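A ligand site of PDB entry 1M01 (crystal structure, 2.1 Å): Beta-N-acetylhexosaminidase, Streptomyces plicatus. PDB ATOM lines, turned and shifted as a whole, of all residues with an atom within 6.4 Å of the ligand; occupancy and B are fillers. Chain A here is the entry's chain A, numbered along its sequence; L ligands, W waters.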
ATOM      1  N   ASP A 165      -7.775  -2.830  14.382  1.00  0.00           N
ATOM      2  CA  ASP A 165      -7.795  -2.298  13.032  1.00  0.00           C
ATOM      3  C   ASP A 165      -7.153  -0.907  13.088  1.00  0.00           C
ATOM      4  O   ASP A 165      -7.711   0.011  13.674  1.00  0.00           O
ATOM      5  CB  ASP A 165      -9.260  -2.194  12.556  1.00  0.00           C
ATOM      6  CG  ASP A 165      -9.422  -1.421  11.245  1.00  0.00           C
ATOM      7  OD1 ASP A 165      -8.414  -0.973  10.651  1.00  0.00           O
ATOM      8  OD2 ASP A 165     -10.583  -1.269  10.812  1.00  0.00           O
ATOM      9  N   ARG A 168      -8.531   1.768   9.321  1.00  0.00           N
ATOM     10  CA  ARG A 168      -9.689   2.656   9.191  1.00  0.00           C
ATOM     11  C   ARG A 168      -9.388   3.975   9.871  1.00  0.00           C
ATOM     12  O   ARG A 168      -9.629   5.036   9.312  1.00  0.00           O
ATOM     13  CB  ARG A 168     -10.937   1.965   9.745  1.00  0.00           C
ATOM     14  CG  ARG A 168     -11.608   1.069   8.697  1.00  0.00           C
ATOM     15  CD  ARG A 168     -10.585   0.274   7.859  1.00  0.00           C
ATOM     16  NE  ARG A 168     -11.255  -0.518   6.832  1.00  0.00           N
ATOM     17  CZ  ARG A 168     -11.847  -1.678   7.061  1.00  0.00           C
ATOM     18  NH1 ARG A 168     -11.832  -2.205   8.279  1.00  0.00           N
ATOM     19  NH2 ARG A 168     -12.494  -2.305   6.083  1.00  0.00           N
ATOM     20  N   HIS A 194      -4.394  -5.354  11.881  1.00  0.00           N
ATOM     21  CA  HIS A 194      -4.914  -5.159  10.528  1.00  0.00           C
ATOM     22  C   HIS A 194      -4.182  -3.926  10.002  1.00  0.00           C
ATOM     23  O   HIS A 194      -4.681  -2.797  10.130  1.00  0.00           O
ATOM     24  CB  HIS A 194      -6.419  -4.934  10.568  1.00  0.00           C
ATOM     25  CG  HIS A 194      -7.100  -5.088   9.248  1.00  0.00           C
ATOM     26  ND1 HIS A 194      -7.391  -6.323   8.695  1.00  0.00           N
ATOM     27  CD2 HIS A 194      -7.576  -4.163   8.369  1.00  0.00           C
ATOM     28  CE1 HIS A 194      -8.005  -6.149   7.548  1.00  0.00           C
ATOM     29  NE2 HIS A 194      -8.131  -4.850   7.325  1.00  0.00           N
ATOM     30  N   ASP A 197      -5.793  -1.690   4.451  1.00  0.00           N
ATOM     31  CA  ASP A 197      -7.150  -1.831   3.968  1.00  0.00           C
ATOM     32  C   ASP A 197      -7.385  -0.756   2.926  1.00  0.00           C
ATOM     33  O   ASP A 197      -6.438  -0.211   2.361  1.00  0.00           O
ATOM     34  CB  ASP A 197      -8.154  -1.713   5.135  1.00  0.00           C
ATOM     35  CG  ASP A 197      -9.432  -2.482   4.881  1.00  0.00           C
ATOM     36  OD1 ASP A 197     -10.225  -2.066   3.998  1.00  0.00           O
ATOM     37  OD2 ASP A 197      -9.649  -3.522   5.542  1.00  0.00           O
ATOM     38  N   ASP A 252      -4.176  -7.437   4.022  1.00  0.00           N
ATOM     39  CA  ASP A 252      -5.338  -7.981   3.334  1.00  0.00           C
ATOM     40  C   ASP A 252      -5.187  -8.003   1.815  1.00  0.00           C
ATOM     41  O   ASP A 252      -4.792  -7.003   1.206  1.00  0.00           O
ATOM     42  CB  ASP A 252      -6.580  -7.164   3.707  1.00  0.00           C
ATOM     43  CG  ASP A 252      -7.852  -7.987   3.682  1.00  0.00           C
ATOM     44  OD1 ASP A 252      -7.906  -9.002   2.950  1.00  0.00           O
ATOM     45  OD2 ASP A 252      -8.809  -7.623   4.391  1.00  0.00           O
ATOM     46  N   HIS A 256      -9.819  -5.353  -0.294  1.00  0.00           N
ATOM     47  CA  HIS A 256      -9.435  -4.381   0.747  1.00  0.00           C
ATOM     48  C   HIS A 256      -8.037  -3.845   0.467  1.00  0.00           C
ATOM     49  O   HIS A 256      -7.241  -3.661   1.394  1.00  0.00           O
ATOM     50  CB  HIS A 256      -9.460  -5.050   2.121  1.00  0.00           C
ATOM     51  CG  HIS A 256     -10.847  -5.298   2.645  1.00  0.00           C
ATOM     52  ND1 HIS A 256     -11.600  -4.299   3.213  1.00  0.00           N
ATOM     53  CD2 HIS A 256     -11.616  -6.406   2.642  1.00  0.00           C
ATOM     54  CE1 HIS A 256     -12.786  -4.792   3.548  1.00  0.00           C
ATOM     55  NE2 HIS A 256     -12.827  -6.066   3.209  1.00  0.00           N
ATOM     56  N   VAL A 282     -17.137  -1.607   2.074  1.00  0.00           N
ATOM     57  CA  VAL A 282     -16.150  -2.656   1.781  1.00  0.00           C
ATOM     58  C   VAL A 282     -16.511  -3.450   0.526  1.00  0.00           C
ATOM     59  O   VAL A 282     -17.673  -3.441   0.105  1.00  0.00           O
ATOM     60  CB  VAL A 282     -16.071  -3.695   2.928  1.00  0.00           C
ATOM     61  CG1 VAL A 282     -15.752  -2.998   4.255  1.00  0.00           C
ATOM     62  CG2 VAL A 282     -17.392  -4.447   3.030  1.00  0.00           C
ATOM     63  N   ASP A 319     -10.782 -11.627   2.719  1.00  0.00           N
ATOM     64  CA  ASP A 319     -12.196 -11.344   2.902  1.00  0.00           C
ATOM     65  C   ASP A 319     -12.738 -10.316   1.920  1.00  0.00           C
ATOM     66  O   ASP A 319     -12.021  -9.421   1.468  1.00  0.00           O
ATOM     67  CB  ASP A 319     -12.431 -10.807   4.314  1.00  0.00           C
ATOM     68  CG  ASP A 319     -11.724  -9.496   4.552  1.00  0.00           C
ATOM     69  OD1 ASP A 319     -10.494  -9.451   4.361  1.00  0.00           O
ATOM     70  OD2 ASP A 319     -12.395  -8.499   4.936  1.00  0.00           O
ATOM     71  N   GLU A 320     -14.011 -10.470   1.597  1.00  0.00           N
ATOM     72  CA  GLU A 320     -14.730  -9.555   0.721  1.00  0.00           C
ATOM     73  C   GLU A 320     -13.999  -9.081  -0.535  1.00  0.00           C
ATOM     74  O   GLU A 320     -13.957  -7.884  -0.836  1.00  0.00           O
ATOM     75  CB  GLU A 320     -15.187  -8.378   1.582  1.00  0.00           C
ATOM     76  CG  GLU A 320     -15.897  -8.881   2.846  1.00  0.00           C
ATOM     77  CD  GLU A 320     -16.118  -7.834   3.923  1.00  0.00           C
ATOM     78  OE1 GLU A 320     -15.320  -6.866   4.022  1.00  0.00           O
ATOM     79  OE2 GLU A 320     -17.086  -7.996   4.697  1.00  0.00           O
ATOM     80  N   TRP A 350      -8.884 -15.124   6.350  1.00  0.00           N
ATOM     81  CA  TRP A 350     -10.278 -15.144   6.790  1.00  0.00           C
ATOM     82  C   TRP A 350     -10.852 -16.431   6.187  1.00  0.00           C
ATOM     83  O   TRP A 350     -10.260 -16.980   5.258  1.00  0.00           O
ATOM     84  CB  TRP A 350     -11.006 -13.889   6.311  1.00  0.00           C
ATOM     85  CG  TRP A 350     -10.454 -12.637   6.953  1.00  0.00           C
ATOM     86  CD1 TRP A 350      -9.613 -11.718   6.379  1.00  0.00           C
ATOM     87  CD2 TRP A 350     -10.664 -12.206   8.300  1.00  0.00           C
ATOM     88  NE1 TRP A 350      -9.285 -10.747   7.296  1.00  0.00           N
ATOM     89  CE2 TRP A 350      -9.911 -11.021   8.478  1.00  0.00           C
ATOM     90  CE3 TRP A 350     -11.413 -12.700   9.379  1.00  0.00           C
ATOM     91  CZ2 TRP A 350      -9.882 -10.326   9.702  1.00  0.00           C
ATOM     92  CZ3 TRP A 350     -11.393 -12.011  10.592  1.00  0.00           C
ATOM     93  CH2 TRP A 350     -10.624 -10.836  10.732  1.00  0.00           C
ATOM     94  N   GLN A 352     -12.794 -17.202   3.950  1.00  0.00           N
ATOM     95  CA  GLN A 352     -13.033 -17.255   2.503  1.00  0.00           C
ATOM     96  C   GLN A 352     -11.923 -18.102   1.894  1.00  0.00           C
ATOM     97  O   GLN A 352     -12.097 -18.708   0.829  1.00  0.00           O
ATOM     98  CB  GLN A 352     -12.988 -15.851   1.876  1.00  0.00           C
ATOM     99  CG  GLN A 352     -14.274 -15.045   2.027  1.00  0.00           C
ATOM    100  CD  GLN A 352     -14.643 -14.820   3.478  1.00  0.00           C
ATOM    101  OE1 GLN A 352     -13.797 -14.438   4.288  1.00  0.00           O
ATOM    102  NE2 GLN A 352     -15.908 -15.048   3.813  1.00  0.00           N
ATOM    103  N   TRP A 367     -15.447 -15.741  10.488  1.00  0.00           N
ATOM    104  CA  TRP A 367     -16.163 -14.578  10.980  1.00  0.00           C
ATOM    105  C   TRP A 367     -17.639 -14.636  10.605  1.00  0.00           C
ATOM    106  O   TRP A 367     -18.318 -13.611  10.531  1.00  0.00           O
ATOM    107  CB  TRP A 367     -15.516 -13.279  10.450  1.00  0.00           C
ATOM    108  CG  TRP A 367     -15.405 -13.200   8.949  1.00  0.00           C
ATOM    109  CD1 TRP A 367     -14.554 -13.904   8.148  1.00  0.00           C
ATOM    110  CD2 TRP A 367     -16.149 -12.341   8.076  1.00  0.00           C
ATOM    111  NE1 TRP A 367     -14.717 -13.536   6.834  1.00  0.00           N
ATOM    112  CE2 TRP A 367     -15.695 -12.579   6.763  1.00  0.00           C
ATOM    113  CE3 TRP A 367     -17.160 -11.388   8.281  1.00  0.00           C
ATOM    114  CZ2 TRP A 367     -16.216 -11.903   5.647  1.00  0.00           C
ATOM    115  CZ3 TRP A 367     -17.682 -10.716   7.179  1.00  0.00           C
ATOM    116  CH2 TRP A 367     -17.206 -10.975   5.870  1.00  0.00           C
ATOM    117  N   ALA A 395     -18.935 -12.749  13.693  1.00  0.00           N
ATOM    118  CA  ALA A 395     -19.279 -11.338  13.628  1.00  0.00           C
ATOM    119  C   ALA A 395     -20.436 -10.951  14.559  1.00  0.00           C
ATOM    120  O   ALA A 395     -20.529  -9.805  14.997  1.00  0.00           O
ATOM    121  CB  ALA A 395     -19.631 -10.948  12.190  1.00  0.00           C
ATOM    122  N   TYR A 399     -17.151  -9.546  17.439  1.00  0.00           N
ATOM    123  CA  TYR A 399     -16.741  -8.329  16.744  1.00  0.00           C
ATOM    124  C   TYR A 399     -17.048  -7.198  17.725  1.00  0.00           C
ATOM    125  O   TYR A 399     -18.211  -6.850  17.959  1.00  0.00           O
ATOM    126  CB  TYR A 399     -17.546  -8.167  15.434  1.00  0.00           C
ATOM    127  CG  TYR A 399     -16.846  -8.752  14.217  1.00  0.00           C
ATOM    128  CD1 TYR A 399     -16.098  -9.929  14.307  1.00  0.00           C
ATOM    129  CD2 TYR A 399     -16.936  -8.124  12.976  1.00  0.00           C
ATOM    130  CE1 TYR A 399     -15.444 -10.466  13.195  1.00  0.00           C
ATOM    131  CE2 TYR A 399     -16.281  -8.657  11.850  1.00  0.00           C
ATOM    132  CZ  TYR A 399     -15.537  -9.814  11.974  1.00  0.00           C
ATOM    133  OH  TYR A 399     -14.868 -10.318  10.881  1.00  0.00           O
ATOM    134  N   ASP A 401     -16.660  -4.113  17.464  1.00  0.00           N
ATOM    135  CA  ASP A 401     -17.140  -2.881  16.863  1.00  0.00           C
ATOM    136  C   ASP A 401     -18.657  -2.957  16.677  1.00  0.00           C
ATOM    137  O   ASP A 401     -19.278  -1.968  16.296  1.00  0.00           O
ATOM    138  CB  ASP A 401     -16.471  -2.650  15.503  1.00  0.00           C
ATOM    139  CG  ASP A 401     -16.800  -3.729  14.496  1.00  0.00           C
ATOM    140  OD1 ASP A 401     -16.665  -4.926  14.837  1.00  0.00           O
ATOM    141  OD2 ASP A 401     -17.163  -3.390  13.353  1.00  0.00           O
ATOM    142  N   MET A 402     -19.252  -4.111  16.936  1.00  0.00           N
ATOM    143  CA  MET A 402     -20.694  -4.246  16.749  1.00  0.00           C
ATOM    144  C   MET A 402     -21.463  -3.609  17.915  1.00  0.00           C
ATOM    145  O   MET A 402     -21.085  -3.753  19.077  1.00  0.00           O
ATOM    146  CB  MET A 402     -21.088  -5.720  16.606  1.00  0.00           C
ATOM    147  CG  MET A 402     -22.235  -5.975  15.618  1.00  0.00           C
ATOM    148  SD  MET A 402     -21.876  -5.378  13.932  1.00  0.00           S
ATOM    149  CE  MET A 402     -20.423  -6.373  13.508  1.00  0.00           C
ATOM    150  N   LEU A 412     -20.996  -0.562  14.449  1.00  0.00           N
ATOM    151  CA  LEU A 412     -21.847  -0.918  13.321  1.00  0.00           C
ATOM    152  C   LEU A 412     -22.947  -1.894  13.735  1.00  0.00           C
ATOM    153  O   LEU A 412     -22.974  -2.393  14.861  1.00  0.00           O
ATOM    154  CB  LEU A 412     -20.985  -1.528  12.202  1.00  0.00           C
ATOM    155  CG  LEU A 412     -19.878  -0.611  11.683  1.00  0.00           C
ATOM    156  CD1 LEU A 412     -19.045  -1.344  10.629  1.00  0.00           C
ATOM    157  CD2 LEU A 412     -20.495   0.659  11.108  1.00  0.00           C
ATOM    158  N   TRP A 414     -24.433  -4.219  11.047  1.00  0.00           N
ATOM    159  CA  TRP A 414     -24.724  -5.121   9.946  1.00  0.00           C
ATOM    160  C   TRP A 414     -24.899  -6.569  10.415  1.00  0.00           C
ATOM    161  O   TRP A 414     -25.617  -7.338   9.774  1.00  0.00           O
ATOM    162  CB  TRP A 414     -23.643  -5.050   8.870  1.00  0.00           C
ATOM    163  CG  TRP A 414     -22.288  -5.514   9.301  1.00  0.00           C
ATOM    164  CD1 TRP A 414     -21.273  -4.747   9.816  1.00  0.00           C
ATOM    165  CD2 TRP A 414     -21.782  -6.858   9.239  1.00  0.00           C
ATOM    166  NE1 TRP A 414     -20.167  -5.524  10.061  1.00  0.00           N
ATOM    167  CE2 TRP A 414     -20.448  -6.822   9.720  1.00  0.00           C
ATOM    168  CE3 TRP A 414     -22.333  -8.075   8.821  1.00  0.00           C
ATOM    169  CZ2 TRP A 414     -19.659  -7.975   9.791  1.00  0.00           C
ATOM    170  CZ3 TRP A 414     -21.535  -9.214   8.897  1.00  0.00           C
ATOM    171  CH2 TRP A 414     -20.213  -9.156   9.375  1.00  0.00           C
ATOM    172  N   TRP A 448     -12.755  -3.510  14.815  1.00  0.00           N
ATOM    173  CA  TRP A 448     -12.665  -2.726  13.584  1.00  0.00           C
ATOM    174  C   TRP A 448     -12.870  -1.257  13.925  1.00  0.00           C
ATOM    175  O   TRP A 448     -13.618  -0.920  14.846  1.00  0.00           O
ATOM    176  CB  TRP A 448     -13.713  -3.200  12.573  1.00  0.00           C
ATOM    177  CG  TRP A 448     -13.537  -4.659  12.210  1.00  0.00           C
ATOM    178  CD1 TRP A 448     -14.245  -5.723  12.690  1.00  0.00           C
ATOM    179  CD2 TRP A 448     -12.555  -5.199  11.314  1.00  0.00           C
ATOM    180  NE1 TRP A 448     -13.774  -6.904  12.146  1.00  0.00           N
ATOM    181  CE2 TRP A 448     -12.736  -6.604  11.293  1.00  0.00           C
ATOM    182  CE3 TRP A 448     -11.551  -4.637  10.515  1.00  0.00           C
ATOM    183  CZ2 TRP A 448     -11.937  -7.458  10.511  1.00  0.00           C
ATOM    184  CZ3 TRP A 448     -10.754  -5.487   9.743  1.00  0.00           C
ATOM    185  CH2 TRP A 448     -10.959  -6.878   9.745  1.00  0.00           C
ATOM    186  N   THR A 449     -12.219  -0.355  13.180  1.00  0.00           N
ATOM    187  CA  THR A 449     -12.319   1.050  13.527  1.00  0.00           C
ATOM    188  C   THR A 449     -12.977   2.068  12.590  1.00  0.00           C
ATOM    189  O   THR A 449     -12.629   3.245  12.616  1.00  0.00           O
ATOM    190  CB  THR A 449     -10.921   1.575  13.938  1.00  0.00           C
ATOM    191  OG1 THR A 449      -9.983   1.381  12.862  1.00  0.00           O
ATOM    192  CG2 THR A 449     -10.417   0.815  15.168  1.00  0.00           C
ATOM    193  N   GLU A 450     -13.929   1.633  11.769  1.00  0.00           N
ATOM    194  CA  GLU A 450     -14.608   2.567  10.888  1.00  0.00           C
ATOM    195  C   GLU A 450     -15.180   3.739  11.699  1.00  0.00           C
ATOM    196  O   GLU A 450     -15.165   4.876  11.231  1.00  0.00           O
ATOM    197  CB  GLU A 450     -15.775   1.907  10.138  1.00  0.00           C
ATOM    198  CG  GLU A 450     -15.370   1.079   8.919  1.00  0.00           C
ATOM    199  CD  GLU A 450     -15.098  -0.365   9.271  1.00  0.00           C
ATOM    200  OE1 GLU A 450     -14.751  -0.645  10.436  1.00  0.00           O
ATOM    201  OE2 GLU A 450     -15.213  -1.223   8.370  1.00  0.00           O
HETATM  202  C1  LIG L   1     -16.313  -6.889   7.998  1.00  0.00           C
HETATM  203  C2  LIG L   1     -15.043  -6.525   7.192  1.00  0.00           C
HETATM  204  C3  LIG L   1     -14.136  -5.482   7.870  1.00  0.00           C
HETATM  205  C4  LIG L   1     -14.967  -4.363   8.508  1.00  0.00           C
HETATM  206  C5  LIG L   1     -15.950  -5.037   9.454  1.00  0.00           C
HETATM  207  C6  LIG L   1     -16.736  -4.087  10.322  1.00  0.00           C
HETATM  208  C7  LIG L   1     -14.230  -8.672   7.924  1.00  0.00           C
HETATM  209  C8  LIG L   1     -13.385  -9.912   7.658  1.00  0.00           C
HETATM  210  N1  LIG L   1     -14.293  -7.747   6.960  1.00  0.00           N
HETATM  211  O1  LIG L   1     -17.255  -7.415   7.138  1.00  0.00           O
HETATM  212  O2  LIG L   1     -13.236  -4.926   6.919  1.00  0.00           O
HETATM  213  O3  LIG L   1     -14.126  -3.470   9.225  1.00  0.00           O
HETATM  214  O4  LIG L   1     -16.896  -5.779   8.680  1.00  0.00           O
HETATM  215  O5  LIG L   1     -17.616  -4.794  11.188  1.00  0.00           O
HETATM  216  O6  LIG L   1     -14.811  -8.553   9.006  1.00  0.00           O
HETATM  217  O   HOH W   1     -11.031  -6.265   6.067  1.00  0.00           O
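A ring nitrogen (NE2) of His 256 lies within hydrogen-bond range of the side-chain carboxylate of Glu 320 (2.7 Å). The side-chain carboxylate (OE2) of Glu 450 lies within salt-bridge range of the guanidinium group (NH1) of Arg 168 (3.5 Å). The side-chain carboxylate (OD2) of Asp 165 lies within salt-bridge range of the guanidinium group (NH1) of Arg 168. NE2 of His 256 is in hydrogen-bond range of OD2 of Asp 319 (3.0 Å). OD1 of Asp 319 sits close to NE1 of Trp 350 (3.4 Å). The side-chain carboxylate (OD2) of Asp 252 lies close to the side-chain carboxylate (OD1) of Asp 319. The backbone carbonyl oxygen of Trp 367 is in hydrogen-bond range of the backbone NH of Ala 395, at 3.3 Å. A ring nitrogen (ND1) of His 256 sits at hydrogen-bond distance from the side-chain carboxylate (OD1) of Asp 197, 2.7 Å away.
An oxygen (O1) of the ligand is in hydrogen-bond range of the side-chain carboxylate (OE2) of Glu 320, at 2.5 Å. The side-chain hydroxyl (OH) of Tyr 399 is in hydrogen-bond range of an oxygen (O6) of the ligand (2.6 Å). The side-chain carboxylate (OD2) of Asp 401 lies within hydrogen-bond range of an oxygen (O5) of the ligand (2.6 Å). The side-chain carboxylate of Glu 450 is in hydrogen-bond range of an oxygen (O3) of the ligand, 2.6 Å away. An oxygen (O3) of the ligand sits at hydrogen-bond distance from the guanidinium group (NH1) of Arg 168 (2.8 Å). The side-chain carboxylate (OD2) of Asp 319 sits at hydrogen-bond distance from a nitrogen (N1) of the ligand. The indole nitrogen (NE1) of Trp 414 lies within hydrogen-bond range of an oxygen (O5) of the ligand, at 2.9 Å.
His 256 touches the ligand (CE1 to O2, 3.4 Å). Trp 350 touches the ligand (CD2 to C8, 3.6 Å). Trp 367 touches the ligand (CZ3 to O1, 3.3 Å). Met 402 touches the ligand. Leu 412 touches the ligand. CE3 of Trp 448 touches O3 of the ligand, at 3.1 Å. Hydrophobic or aromatic side chains that line the ligand: His 256, Trp 350, Trp 367, Tyr 399, Met 402, Leu 412, Trp 414 and Trp 448. Within 4 Å of the ligand: Arg 168, His 256, Asp 319, Glu 320, Trp 350, Trp 367, Tyr 399, Asp 401, Met 402, Leu 412, Trp 414, Trp 448 and Glu 450. Along chain A the residues within 4 Å of the ligand span positions 168 to 450.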
